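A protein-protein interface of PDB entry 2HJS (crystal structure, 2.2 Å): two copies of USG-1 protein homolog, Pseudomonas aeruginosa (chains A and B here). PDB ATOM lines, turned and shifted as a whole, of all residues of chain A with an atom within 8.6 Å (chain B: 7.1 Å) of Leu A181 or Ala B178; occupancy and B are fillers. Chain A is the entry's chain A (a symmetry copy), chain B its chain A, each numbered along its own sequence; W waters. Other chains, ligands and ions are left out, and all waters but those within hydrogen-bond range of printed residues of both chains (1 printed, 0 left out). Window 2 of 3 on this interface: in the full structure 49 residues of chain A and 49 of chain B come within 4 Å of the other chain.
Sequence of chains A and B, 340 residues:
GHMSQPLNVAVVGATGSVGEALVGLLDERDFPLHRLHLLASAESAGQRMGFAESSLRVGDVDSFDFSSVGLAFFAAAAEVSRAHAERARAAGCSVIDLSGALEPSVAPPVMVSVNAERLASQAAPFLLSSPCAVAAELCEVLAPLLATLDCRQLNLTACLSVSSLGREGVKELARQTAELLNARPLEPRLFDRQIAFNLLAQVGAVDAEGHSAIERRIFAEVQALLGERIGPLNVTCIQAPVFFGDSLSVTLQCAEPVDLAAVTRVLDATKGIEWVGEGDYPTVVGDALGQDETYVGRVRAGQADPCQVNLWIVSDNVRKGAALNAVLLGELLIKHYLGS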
ATOM      1  N   ALA A 174     -29.185  -1.706 -18.724  1.00  0.00           N
ATOM      2  CA  ALA A 174     -28.187  -2.572 -19.360  1.00  0.00           C
ATOM      3  C   ALA A 174     -28.390  -2.655 -20.882  1.00  0.00           C
ATOM      4  O   ALA A 174     -27.426  -2.597 -21.645  1.00  0.00           O
ATOM      5  CB  ALA A 174     -28.217  -3.973 -18.728  1.00  0.00           C
ATOM      6  N   ARG A 175     -29.646  -2.777 -21.313  1.00  0.00           N
ATOM      7  CA  ARG A 175     -29.982  -2.925 -22.736  1.00  0.00           C
ATOM      8  C   ARG A 175     -29.700  -1.642 -23.525  1.00  0.00           C
ATOM      9  O   ARG A 175     -29.071  -1.682 -24.580  1.00  0.00           O
ATOM     10  CB  ARG A 175     -31.442  -3.367 -22.908  1.00  0.00           C
ATOM     11  CG  ARG A 175     -31.801  -3.769 -24.330  1.00  0.00           C
ATOM     12  CD  ARG A 175     -33.288  -4.144 -24.495  1.00  0.00           C
ATOM     13  NE  ARG A 175     -34.166  -3.157 -23.870  1.00  0.00           N
ATOM     14  CZ  ARG A 175     -34.554  -2.013 -24.437  1.00  0.00           C
ATOM     15  NH1 ARG A 175     -34.154  -1.692 -25.667  1.00  0.00           N
ATOM     16  NH2 ARG A 175     -35.341  -1.177 -23.756  1.00  0.00           N
ATOM     17  N   GLN A 176     -30.162  -0.508 -22.998  1.00  0.00           N
ATOM     18  CA  GLN A 176     -29.900   0.796 -23.610  1.00  0.00           C
ATOM     19  C   GLN A 176     -28.406   1.072 -23.685  1.00  0.00           C
ATOM     20  O   GLN A 176     -27.928   1.563 -24.700  1.00  0.00           O
ATOM     21  CB  GLN A 176     -30.578   1.921 -22.828  1.00  0.00           C
ATOM     22  CG  GLN A 176     -32.075   2.050 -23.030  1.00  0.00           C
ATOM     23  CD  GLN A 176     -32.583   3.438 -22.668  1.00  0.00           C
ATOM     24  OE1 GLN A 176     -31.799   4.387 -22.545  1.00  0.00           O
ATOM     25  NE2 GLN A 176     -33.897   3.570 -22.499  1.00  0.00           N
ATOM     26  N   THR A 177     -27.676   0.759 -22.611  1.00  0.00           N
ATOM     27  CA  THR A 177     -26.242   1.040 -22.559  1.00  0.00           C
ATOM     28  C   THR A 177     -25.528   0.247 -23.646  1.00  0.00           C
ATOM     29  O   THR A 177     -24.680   0.794 -24.356  1.00  0.00           O
ATOM     30  CB  THR A 177     -25.618   0.774 -21.158  1.00  0.00           C
ATOM     31  OG1 THR A 177     -26.291   1.561 -20.165  1.00  0.00           O
ATOM     32  CG2 THR A 177     -24.157   1.172 -21.141  1.00  0.00           C
ATOM     33  N   ALA A 178     -25.915  -1.021 -23.802  1.00  0.00           N
ATOM     34  CA  ALA A 178     -25.319  -1.914 -24.792  1.00  0.00           C
ATOM     35  C   ALA A 178     -25.606  -1.461 -26.223  1.00  0.00           C
ATOM     36  O   ALA A 178     -24.689  -1.405 -27.048  1.00  0.00           O
ATOM     37  CB  ALA A 178     -25.810  -3.332 -24.576  1.00  0.00           C
ATOM     38  N   GLU A 179     -26.870  -1.145 -26.513  1.00  0.00           N
ATOM     39  CA  GLU A 179     -27.264  -0.629 -27.817  1.00  0.00           C
ATOM     40  C   GLU A 179     -26.370   0.542 -28.238  1.00  0.00           C
ATOM     41  O   GLU A 179     -25.873   0.571 -29.358  1.00  0.00           O
ATOM     42  CB  GLU A 179     -28.733  -0.204 -27.815  1.00  0.00           C
ATOM     43  CG  GLU A 179     -29.719  -1.352 -27.987  1.00  0.00           C
ATOM     44  CD  GLU A 179     -31.123  -1.047 -27.437  1.00  0.00           C
ATOM     45  OE1 GLU A 179     -31.372   0.092 -26.949  1.00  0.00           O
ATOM     46  OE2 GLU A 179     -31.982  -1.963 -27.497  1.00  0.00           O
ATOM     47  N   LEU A 180     -26.147   1.491 -27.329  1.00  0.00           N
ATOM     48  CA  LEU A 180     -25.326   2.660 -27.630  1.00  0.00           C
ATOM     49  C   LEU A 180     -23.853   2.317 -27.842  1.00  0.00           C
ATOM     50  O   LEU A 180     -23.214   2.851 -28.760  1.00  0.00           O
ATOM     51  CB  LEU A 180     -25.452   3.715 -26.533  1.00  0.00           C
ATOM     52  CG  LEU A 180     -26.787   4.429 -26.384  1.00  0.00           C
ATOM     53  CD1 LEU A 180     -26.759   5.221 -25.112  1.00  0.00           C
ATOM     54  CD2 LEU A 180     -27.084   5.333 -27.591  1.00  0.00           C
ATOM     55  N   LEU A 181     -23.327   1.423 -27.007  1.00  0.00           N
ATOM     56  CA  LEU A 181     -21.907   1.086 -27.054  1.00  0.00           C
ATOM     57  C   LEU A 181     -21.484   0.351 -28.323  1.00  0.00           C
ATOM     58  O   LEU A 181     -20.380   0.572 -28.823  1.00  0.00           O
ATOM     59  CB  LEU A 181     -21.452   0.352 -25.786  1.00  0.00           C
ATOM     60  CG  LEU A 181     -21.180   1.259 -24.572  1.00  0.00           C
ATOM     61  CD1 LEU A 181     -20.622   0.448 -23.413  1.00  0.00           C
ATOM     62  CD2 LEU A 181     -20.249   2.437 -24.889  1.00  0.00           C
ATOM     63  N   ASN A 182     -22.343  -0.508 -28.860  1.00  0.00           N
ATOM     64  CA  ASN A 182     -22.047  -1.087 -30.168  1.00  0.00           C
ATOM     65  C   ASN A 182     -22.860  -0.477 -31.328  1.00  0.00           C
ATOM     66  O   ASN A 182     -23.181  -1.152 -32.314  1.00  0.00           O
ATOM     67  CB  ASN A 182     -22.044  -2.626 -30.142  1.00  0.00           C
ATOM     68  CG  ASN A 182     -23.258  -3.209 -29.467  1.00  0.00           C
ATOM     69  OD1 ASN A 182     -23.160  -3.778 -28.376  1.00  0.00           O
ATOM     70  ND2 ASN A 182     -24.414  -3.087 -30.117  1.00  0.00           N
ATOM     71  N   ALA A 183     -23.154   0.820 -31.184  1.00  0.00           N
ATOM     72  CA  ALA A 183     -23.733   1.675 -32.236  1.00  0.00           C
ATOM     73  C   ALA A 183     -24.989   1.117 -32.930  1.00  0.00           C
ATOM     74  O   ALA A 183     -25.082   1.099 -34.170  1.00  0.00           O
ATOM     75  CB  ALA A 183     -22.652   2.078 -33.267  1.00  0.00           C
ATOM     76  N   ARG A 184     -25.947   0.664 -32.120  1.00  0.00           N
ATOM     77  CA  ARG A 184     -27.242   0.205 -32.624  1.00  0.00           C
ATOM     78  C   ARG A 184     -28.364   1.201 -32.291  1.00  0.00           C
ATOM     79  O   ARG A 184     -28.228   1.990 -31.343  1.00  0.00           O
ATOM     80  CB  ARG A 184     -27.563  -1.201 -32.107  1.00  0.00           C
ATOM     81  CG  ARG A 184     -26.879  -2.307 -32.909  1.00  0.00           C
ATOM     82  CD  ARG A 184     -27.415  -3.698 -32.568  1.00  0.00           C
ATOM     83  NE  ARG A 184     -27.205  -4.043 -31.159  1.00  0.00           N
ATOM     84  CZ  ARG A 184     -28.165  -4.069 -30.232  1.00  0.00           C
ATOM     85  NH1 ARG A 184     -27.870  -4.394 -28.973  1.00  0.00           N
ATOM     86  NH2 ARG A 184     -29.424  -3.776 -30.559  1.00  0.00           N
ATOM     87  N   LEU A 186     -31.067   3.079 -30.655  1.00  0.00           N
ATOM     88  CA  LEU A 186     -31.618   3.092 -29.300  1.00  0.00           C
ATOM     89  C   LEU A 186     -33.141   3.027 -29.348  1.00  0.00           C
ATOM     90  O   LEU A 186     -33.786   3.823 -30.042  1.00  0.00           O
ATOM     91  CB  LEU A 186     -31.171   4.327 -28.515  1.00  0.00           C
ATOM     92  CG  LEU A 186     -31.685   4.359 -27.073  1.00  0.00           C
ATOM     93  CD1 LEU A 186     -30.636   3.828 -26.122  1.00  0.00           C
ATOM     94  CD2 LEU A 186     -32.112   5.763 -26.696  1.00  0.00           C
ATOM     95  N   ALA A 196     -29.642   5.594 -20.426  1.00  0.00           N
ATOM     96  CA  ALA A 196     -28.226   5.289 -20.498  1.00  0.00           C
ATOM     97  C   ALA A 196     -27.404   6.590 -20.528  1.00  0.00           C
ATOM     98  O   ALA A 196     -27.746   7.533 -21.255  1.00  0.00           O
ATOM     99  CB  ALA A 196     -27.931   4.424 -21.740  1.00  0.00           C
ATOM    100  N   PHE A 197     -26.342   6.640 -19.723  1.00  0.00           N
ATOM    101  CA  PHE A 197     -25.467   7.820 -19.656  1.00  0.00           C
ATOM    102  C   PHE A 197     -26.250   9.155 -19.514  1.00  0.00           C
ATOM    103  O   PHE A 197     -25.839  10.180 -20.036  1.00  0.00           O
ATOM    104  CB  PHE A 197     -24.538   7.859 -20.881  1.00  0.00           C
ATOM    105  CG  PHE A 197     -23.786   6.577 -21.129  1.00  0.00           C
ATOM    106  CD1 PHE A 197     -22.802   6.145 -20.241  1.00  0.00           C
ATOM    107  CD2 PHE A 197     -24.042   5.826 -22.270  1.00  0.00           C
ATOM    108  CE1 PHE A 197     -22.081   4.968 -20.482  1.00  0.00           C
ATOM    109  CE2 PHE A 197     -23.330   4.641 -22.531  1.00  0.00           C
ATOM    110  CZ  PHE A 197     -22.351   4.213 -21.628  1.00  0.00           C
ATOM    111  N   GLU B 172     -12.134   7.085 -20.499  1.00  0.00           N
ATOM    112  CA  GLU B 172     -12.128   6.224 -19.315  1.00  0.00           C
ATOM    113  C   GLU B 172     -13.517   5.638 -19.056  1.00  0.00           C
ATOM    114  O   GLU B 172     -13.656   4.439 -18.792  1.00  0.00           O
ATOM    115  CB  GLU B 172     -11.628   7.019 -18.102  1.00  0.00           C
ATOM    116  CG  GLU B 172     -11.596   6.259 -16.772  1.00  0.00           C
ATOM    117  CD  GLU B 172     -10.423   5.308 -16.642  1.00  0.00           C
ATOM    118  OE1 GLU B 172      -9.517   5.339 -17.505  1.00  0.00           O
ATOM    119  OE2 GLU B 172     -10.400   4.525 -15.670  1.00  0.00           O
ATOM    120  N   LEU B 173     -14.538   6.480 -19.162  1.00  0.00           N
ATOM    121  CA  LEU B 173     -15.902   6.042 -18.923  1.00  0.00           C
ATOM    122  C   LEU B 173     -16.354   5.015 -19.946  1.00  0.00           C
ATOM    123  O   LEU B 173     -16.866   3.956 -19.574  1.00  0.00           O
ATOM    124  CB  LEU B 173     -16.883   7.222 -18.875  1.00  0.00           C
ATOM    125  CG  LEU B 173     -18.341   6.818 -18.599  1.00  0.00           C
ATOM    126  CD1 LEU B 173     -18.531   6.220 -17.174  1.00  0.00           C
ATOM    127  CD2 LEU B 173     -19.270   7.979 -18.820  1.00  0.00           C
ATOM    128  N   ALA B 174     -16.155   5.325 -21.228  1.00  0.00           N
ATOM    129  CA  ALA B 174     -16.515   4.397 -22.306  1.00  0.00           C
ATOM    130  C   ALA B 174     -15.801   3.044 -22.156  1.00  0.00           C
ATOM    131  O   ALA B 174     -16.411   1.991 -22.344  1.00  0.00           O
ATOM    132  CB  ALA B 174     -16.210   5.027 -23.675  1.00  0.00           C
ATOM    133  N   ARG B 175     -14.515   3.081 -21.807  1.00  0.00           N
ATOM    134  CA  ARG B 175     -13.694   1.868 -21.684  1.00  0.00           C
ATOM    135  C   ARG B 175     -14.125   1.005 -20.494  1.00  0.00           C
ATOM    136  O   ARG B 175     -14.311  -0.202 -20.631  1.00  0.00           O
ATOM    137  CB  ARG B 175     -12.203   2.225 -21.594  1.00  0.00           C
ATOM    138  CG  ARG B 175     -11.274   1.026 -21.701  1.00  0.00           C
ATOM    139  CD  ARG B 175      -9.786   1.398 -21.539  1.00  0.00           C
ATOM    140  NE  ARG B 175      -9.570   2.271 -20.387  1.00  0.00           N
ATOM    141  CZ  ARG B 175      -9.441   1.852 -19.127  1.00  0.00           C
ATOM    142  NH1 ARG B 175      -9.493   0.554 -18.831  1.00  0.00           N
ATOM    143  NH2 ARG B 175      -9.270   2.749 -18.153  1.00  0.00           N
ATOM    144  N   GLN B 176     -14.292   1.638 -19.332  1.00  0.00           N
ATOM    145  CA  GLN B 176     -14.772   0.948 -18.134  1.00  0.00           C
ATOM    146  C   GLN B 176     -16.153   0.351 -18.366  1.00  0.00           C
ATOM    147  O   GLN B 176     -16.404  -0.777 -17.959  1.00  0.00           O
ATOM    148  CB  GLN B 176     -14.831   1.895 -16.935  1.00  0.00           C
ATOM    149  CG  GLN B 176     -13.499   2.226 -16.294  1.00  0.00           C
ATOM    150  CD  GLN B 176     -13.660   2.715 -14.862  1.00  0.00           C
ATOM    151  OE1 GLN B 176     -14.718   2.539 -14.248  1.00  0.00           O
ATOM    152  NE2 GLN B 176     -12.610   3.330 -14.318  1.00  0.00           N
ATOM    153  N   THR B 177     -17.041   1.108 -19.015  1.00  0.00           N
ATOM    154  CA  THR B 177     -18.412   0.651 -19.235  1.00  0.00           C
ATOM    155  C   THR B 177     -18.398  -0.601 -20.102  1.00  0.00           C
ATOM    156  O   THR B 177     -19.096  -1.573 -19.798  1.00  0.00           O
ATOM    157  CB  THR B 177     -19.333   1.751 -19.839  1.00  0.00           C
ATOM    158  OG1 THR B 177     -19.350   2.901 -18.982  1.00  0.00           O
ATOM    159  CG2 THR B 177     -20.758   1.249 -19.955  1.00  0.00           C
ATOM    160  N   ALA B 178     -17.564  -0.588 -21.145  1.00  0.00           N
ATOM    161  CA  ALA B 178     -17.444  -1.705 -22.077  1.00  0.00           C
ATOM    162  C   ALA B 178     -16.873  -2.955 -21.407  1.00  0.00           C
ATOM    163  O   ALA B 178     -17.421  -4.049 -21.573  1.00  0.00           O
ATOM    164  CB  ALA B 178     -16.591  -1.304 -23.264  1.00  0.00           C
ATOM    165  N   GLU B 179     -15.781  -2.791 -20.658  1.00  0.00           N
ATOM    166  CA  GLU B 179     -15.181  -3.887 -19.907  1.00  0.00           C
ATOM    167  C   GLU B 179     -16.233  -4.616 -19.064  1.00  0.00           C
ATOM    168  O   GLU B 179     -16.304  -5.839 -19.085  1.00  0.00           O
ATOM    169  CB  GLU B 179     -14.044  -3.379 -19.019  1.00  0.00           C
ATOM    170  CG  GLU B 179     -12.722  -3.174 -19.747  1.00  0.00           C
ATOM    171  CD  GLU B 179     -11.783  -2.176 -19.051  1.00  0.00           C
ATOM    172  OE1 GLU B 179     -12.125  -1.653 -17.953  1.00  0.00           O
ATOM    173  OE2 GLU B 179     -10.689  -1.913 -19.617  1.00  0.00           O
ATOM    174  N   LEU B 180     -17.062  -3.860 -18.345  1.00  0.00           N
ATOM    175  CA  LEU B 180     -18.089  -4.451 -17.491  1.00  0.00           C
ATOM    176  C   LEU B 180     -19.188  -5.157 -18.282  1.00  0.00           C
ATOM    177  O   LEU B 180     -19.629  -6.251 -17.898  1.00  0.00           O
ATOM    178  CB  LEU B 180     -18.712  -3.400 -16.576  1.00  0.00           C
ATOM    179  CG  LEU B 180     -17.842  -2.809 -15.477  1.00  0.00           C
ATOM    180  CD1 LEU B 180     -18.566  -1.641 -14.878  1.00  0.00           C
ATOM    181  CD2 LEU B 180     -17.494  -3.852 -14.405  1.00  0.00           C
ATOM    182  N   LEU B 181     -19.616  -4.541 -19.383  1.00  0.00           N
ATOM    183  CA  LEU B 181     -20.725  -5.074 -20.167  1.00  0.00           C
ATOM    184  C   LEU B 181     -20.417  -6.397 -20.863  1.00  0.00           C
ATOM    185  O   LEU B 181     -21.294  -7.255 -20.972  1.00  0.00           O
ATOM    186  CB  LEU B 181     -21.290  -4.031 -21.138  1.00  0.00           C
ATOM    187  CG  LEU B 181     -22.250  -3.005 -20.507  1.00  0.00           C
ATOM    188  CD1 LEU B 181     -22.842  -2.099 -21.574  1.00  0.00           C
ATOM    189  CD2 LEU B 181     -23.371  -3.651 -19.681  1.00  0.00           C
ATOM    190  N   ASN B 182     -19.184  -6.583 -21.325  1.00  0.00           N
ATOM    191  CA  ASN B 182     -18.806  -7.900 -21.830  1.00  0.00           C
ATOM    192  C   ASN B 182     -17.921  -8.715 -20.865  1.00  0.00           C
ATOM    193  O   ASN B 182     -17.075  -9.515 -21.287  1.00  0.00           O
ATOM    194  CB  ASN B 182     -18.280  -7.848 -23.275  1.00  0.00           C
ATOM    195  CG  ASN B 182     -17.239  -6.780 -23.487  1.00  0.00           C
ATOM    196  OD1 ASN B 182     -17.489  -5.780 -24.168  1.00  0.00           O
ATOM    197  ND2 ASN B 182     -16.052  -6.987 -22.919  1.00  0.00           N
ATOM    198  N   ALA B 183     -18.164  -8.504 -19.567  1.00  0.00           N
ATOM    199  CA  ALA B 183     -17.604  -9.303 -18.462  1.00  0.00           C
ATOM    200  C   ALA B 183     -16.078  -9.505 -18.494  1.00  0.00           C
ATOM    201  O   ALA B 183     -15.577 -10.634 -18.350  1.00  0.00           O
ATOM    202  CB  ALA B 183     -18.347 -10.654 -18.337  1.00  0.00           C
ATOM    203  N   ARG B 184     -15.351  -8.402 -18.684  1.00  0.00           N
ATOM    204  CA  ARG B 184     -13.888  -8.414 -18.629  1.00  0.00           C
ATOM    205  C   ARG B 184     -13.364  -7.730 -17.356  1.00  0.00           C
ATOM    206  O   ARG B 184     -14.075  -6.904 -16.762  1.00  0.00           O
ATOM    207  CB  ARG B 184     -13.289  -7.790 -19.893  1.00  0.00           C
ATOM    208  CG  ARG B 184     -13.234  -8.758 -21.074  1.00  0.00           C
ATOM    209  CD  ARG B 184     -12.393  -8.225 -22.234  1.00  0.00           C
ATOM    210  NE  ARG B 184     -12.926  -6.971 -22.775  1.00  0.00           N
ATOM    211  CZ  ARG B 184     -12.385  -5.767 -22.576  1.00  0.00           C
ATOM    212  NH1 ARG B 184     -12.951  -4.685 -23.111  1.00  0.00           N
ATOM    213  NH2 ARG B 184     -11.277  -5.640 -21.848  1.00  0.00           N
ATOM    214  N   ALA B 196     -17.735   3.748 -14.058  1.00  0.00           N
ATOM    215  CA  ALA B 196     -18.845   3.192 -14.809  1.00  0.00           C
ATOM    216  C   ALA B 196     -20.009   2.851 -13.860  1.00  0.00           C
ATOM    217  O   ALA B 196     -19.796   2.272 -12.787  1.00  0.00           O
ATOM    218  CB  ALA B 196     -18.386   1.943 -15.587  1.00  0.00           C
ATOM    219  N   PHE B 197     -21.225   3.234 -14.252  1.00  0.00           N
ATOM    220  CA  PHE B 197     -22.425   2.969 -13.446  1.00  0.00           C
ATOM    221  C   PHE B 197     -22.252   3.350 -11.948  1.00  0.00           C
ATOM    222  O   PHE B 197     -22.797   2.697 -11.070  1.00  0.00           O
ATOM    223  CB  PHE B 197     -22.844   1.496 -13.590  1.00  0.00           C
ATOM    224  CG  PHE B 197     -22.972   1.026 -15.016  1.00  0.00           C
ATOM    225  CD1 PHE B 197     -23.980   1.523 -15.843  1.00  0.00           C
ATOM    226  CD2 PHE B 197     -22.106   0.061 -15.515  1.00  0.00           C
ATOM    227  CE1 PHE B 197     -24.120   1.068 -17.160  1.00  0.00           C
ATOM    228  CE2 PHE B 197     -22.229  -0.409 -16.835  1.00  0.00           C
ATOM    229  CZ  PHE B 197     -23.238   0.103 -17.658  1.00  0.00           C
ATOM    230  N   PHE B 243     -21.471  11.203 -20.206  1.00  0.00           N
ATOM    231  CA  PHE B 243     -20.350  11.715 -21.028  1.00  0.00           C
ATOM    232  C   PHE B 243     -20.229  13.236 -21.059  1.00  0.00           C
ATOM    233  O   PHE B 243     -19.164  13.771 -20.773  1.00  0.00           O
ATOM    234  CB  PHE B 243     -20.399  11.156 -22.446  1.00  0.00           C
ATOM    235  CG  PHE B 243     -20.074   9.691 -22.521  1.00  0.00           C
ATOM    236  CD1 PHE B 243     -21.069   8.770 -22.782  1.00  0.00           C
ATOM    237  CD2 PHE B 243     -18.769   9.236 -22.308  1.00  0.00           C
ATOM    238  CE1 PHE B 243     -20.789   7.394 -22.853  1.00  0.00           C
ATOM    239  CE2 PHE B 243     -18.475   7.859 -22.365  1.00  0.00           C
ATOM    240  CZ  PHE B 243     -19.487   6.941 -22.639  1.00  0.00           C
HETATM  241  O   HOH W   1     -23.923  11.040 -21.718  1.00  0.00           O
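O of Ala B178 lies close to OD1 of Asn B182. The side-chain hydroxyl (OG1) of Thr B177 is in hydrogen-bond range of the backbone carbonyl oxygen (O) of Leu B173, 2.8 Å away. O of Ala A178 sits close to OD1 of Asn A182.
Thr A177 touches Thr B177 (CG2 to CG2, 3.6 Å). Thr A177 touches Leu B181. OG1 of Thr A177 touches CE1 of Phe B197, 3.7 Å away. Ala A178 touches Leu B181. Thr B177 touches Leu A181. Ala B178 touches Leu A181 (N to CD1, 3.9 Å). CD1 of Leu A181 touches CD1 of Leu B181, 3.8 Å away. Phe A197 touches Thr B177. Phe A197 touches Phe B243 (CD1 to CE1, 3.5 Å).
Printed residues of chain B within 4 Å of Thr A177: Thr B177 (3.6 Å), Leu B181 (3.6 Å) and Phe B197 (3.7 Å). Printed residues of chain B within 4 Å of Phe A197: Thr B177 (3.7 Å) and Phe B243 (3.5 Å). Glu B172 touches none of the printed residues of chain A. Of the printed residues of chain A, Thr B177 touches Thr A177, Leu A181 and Phe A197. Printed residues of chain A within 4 Å of Leu B181: Thr A177 (3.6 Å), Ala A178 (3.9 Å) and Leu A181 (3.8 Å). Printed residues of chain A within 4 Å of Phe B243: Phe A197 (3.5 Å). The nearest residue of chain B that does not touch Leu A181 is Ala B174 (4.6 Å). The nearest printed residue of chain A that does not touch Ala B178 is Phe A197 (6.8 Å).
Hydrophobic or aromatic side chains of chain A that line the printed part of chain B: Leu A181 and Phe A197. Along chain A the printed residues that touch a printed residue of chain B span positions 177 to 197. Of the 16 printed residues of chain B, 5 touch a printed residue of chain A. Hydrophobic or aromatic side chains of chain B within 4 Å of the printed part of chain A: Leu B181, Phe B197 and Phe B243. Along chain B the printed residues that touch a printed residue of chain A span positions 177 to 243. Among the printed residues, no Asp or Glu carboxylate lies within 4 Å of a Lys or Arg side-chain nitrogen of the other chain.
Thr B177 touches its own counterpart, Thr A177. Thr A177 touches Leu B181, and with the chains exchanged Leu A181 touches Thr B177. Ala A178 touches Leu B181, and with the chains exchanged Leu A181 touches Ala B178. Leu A181 touches its own counterpart, Leu B181. Positions printed for both chains: 174, 175, 176, 177, 178, 179, 180, 181, 182, 183, 184, 196 and 197. Of the 9 pairs that touch across the chains among the printed residues, 8 have their exchanged pair printed and touching as well.
Water W1 bridges O of Phe A197 (2.7 Å) and N of Phe B243 (2.9 Å).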
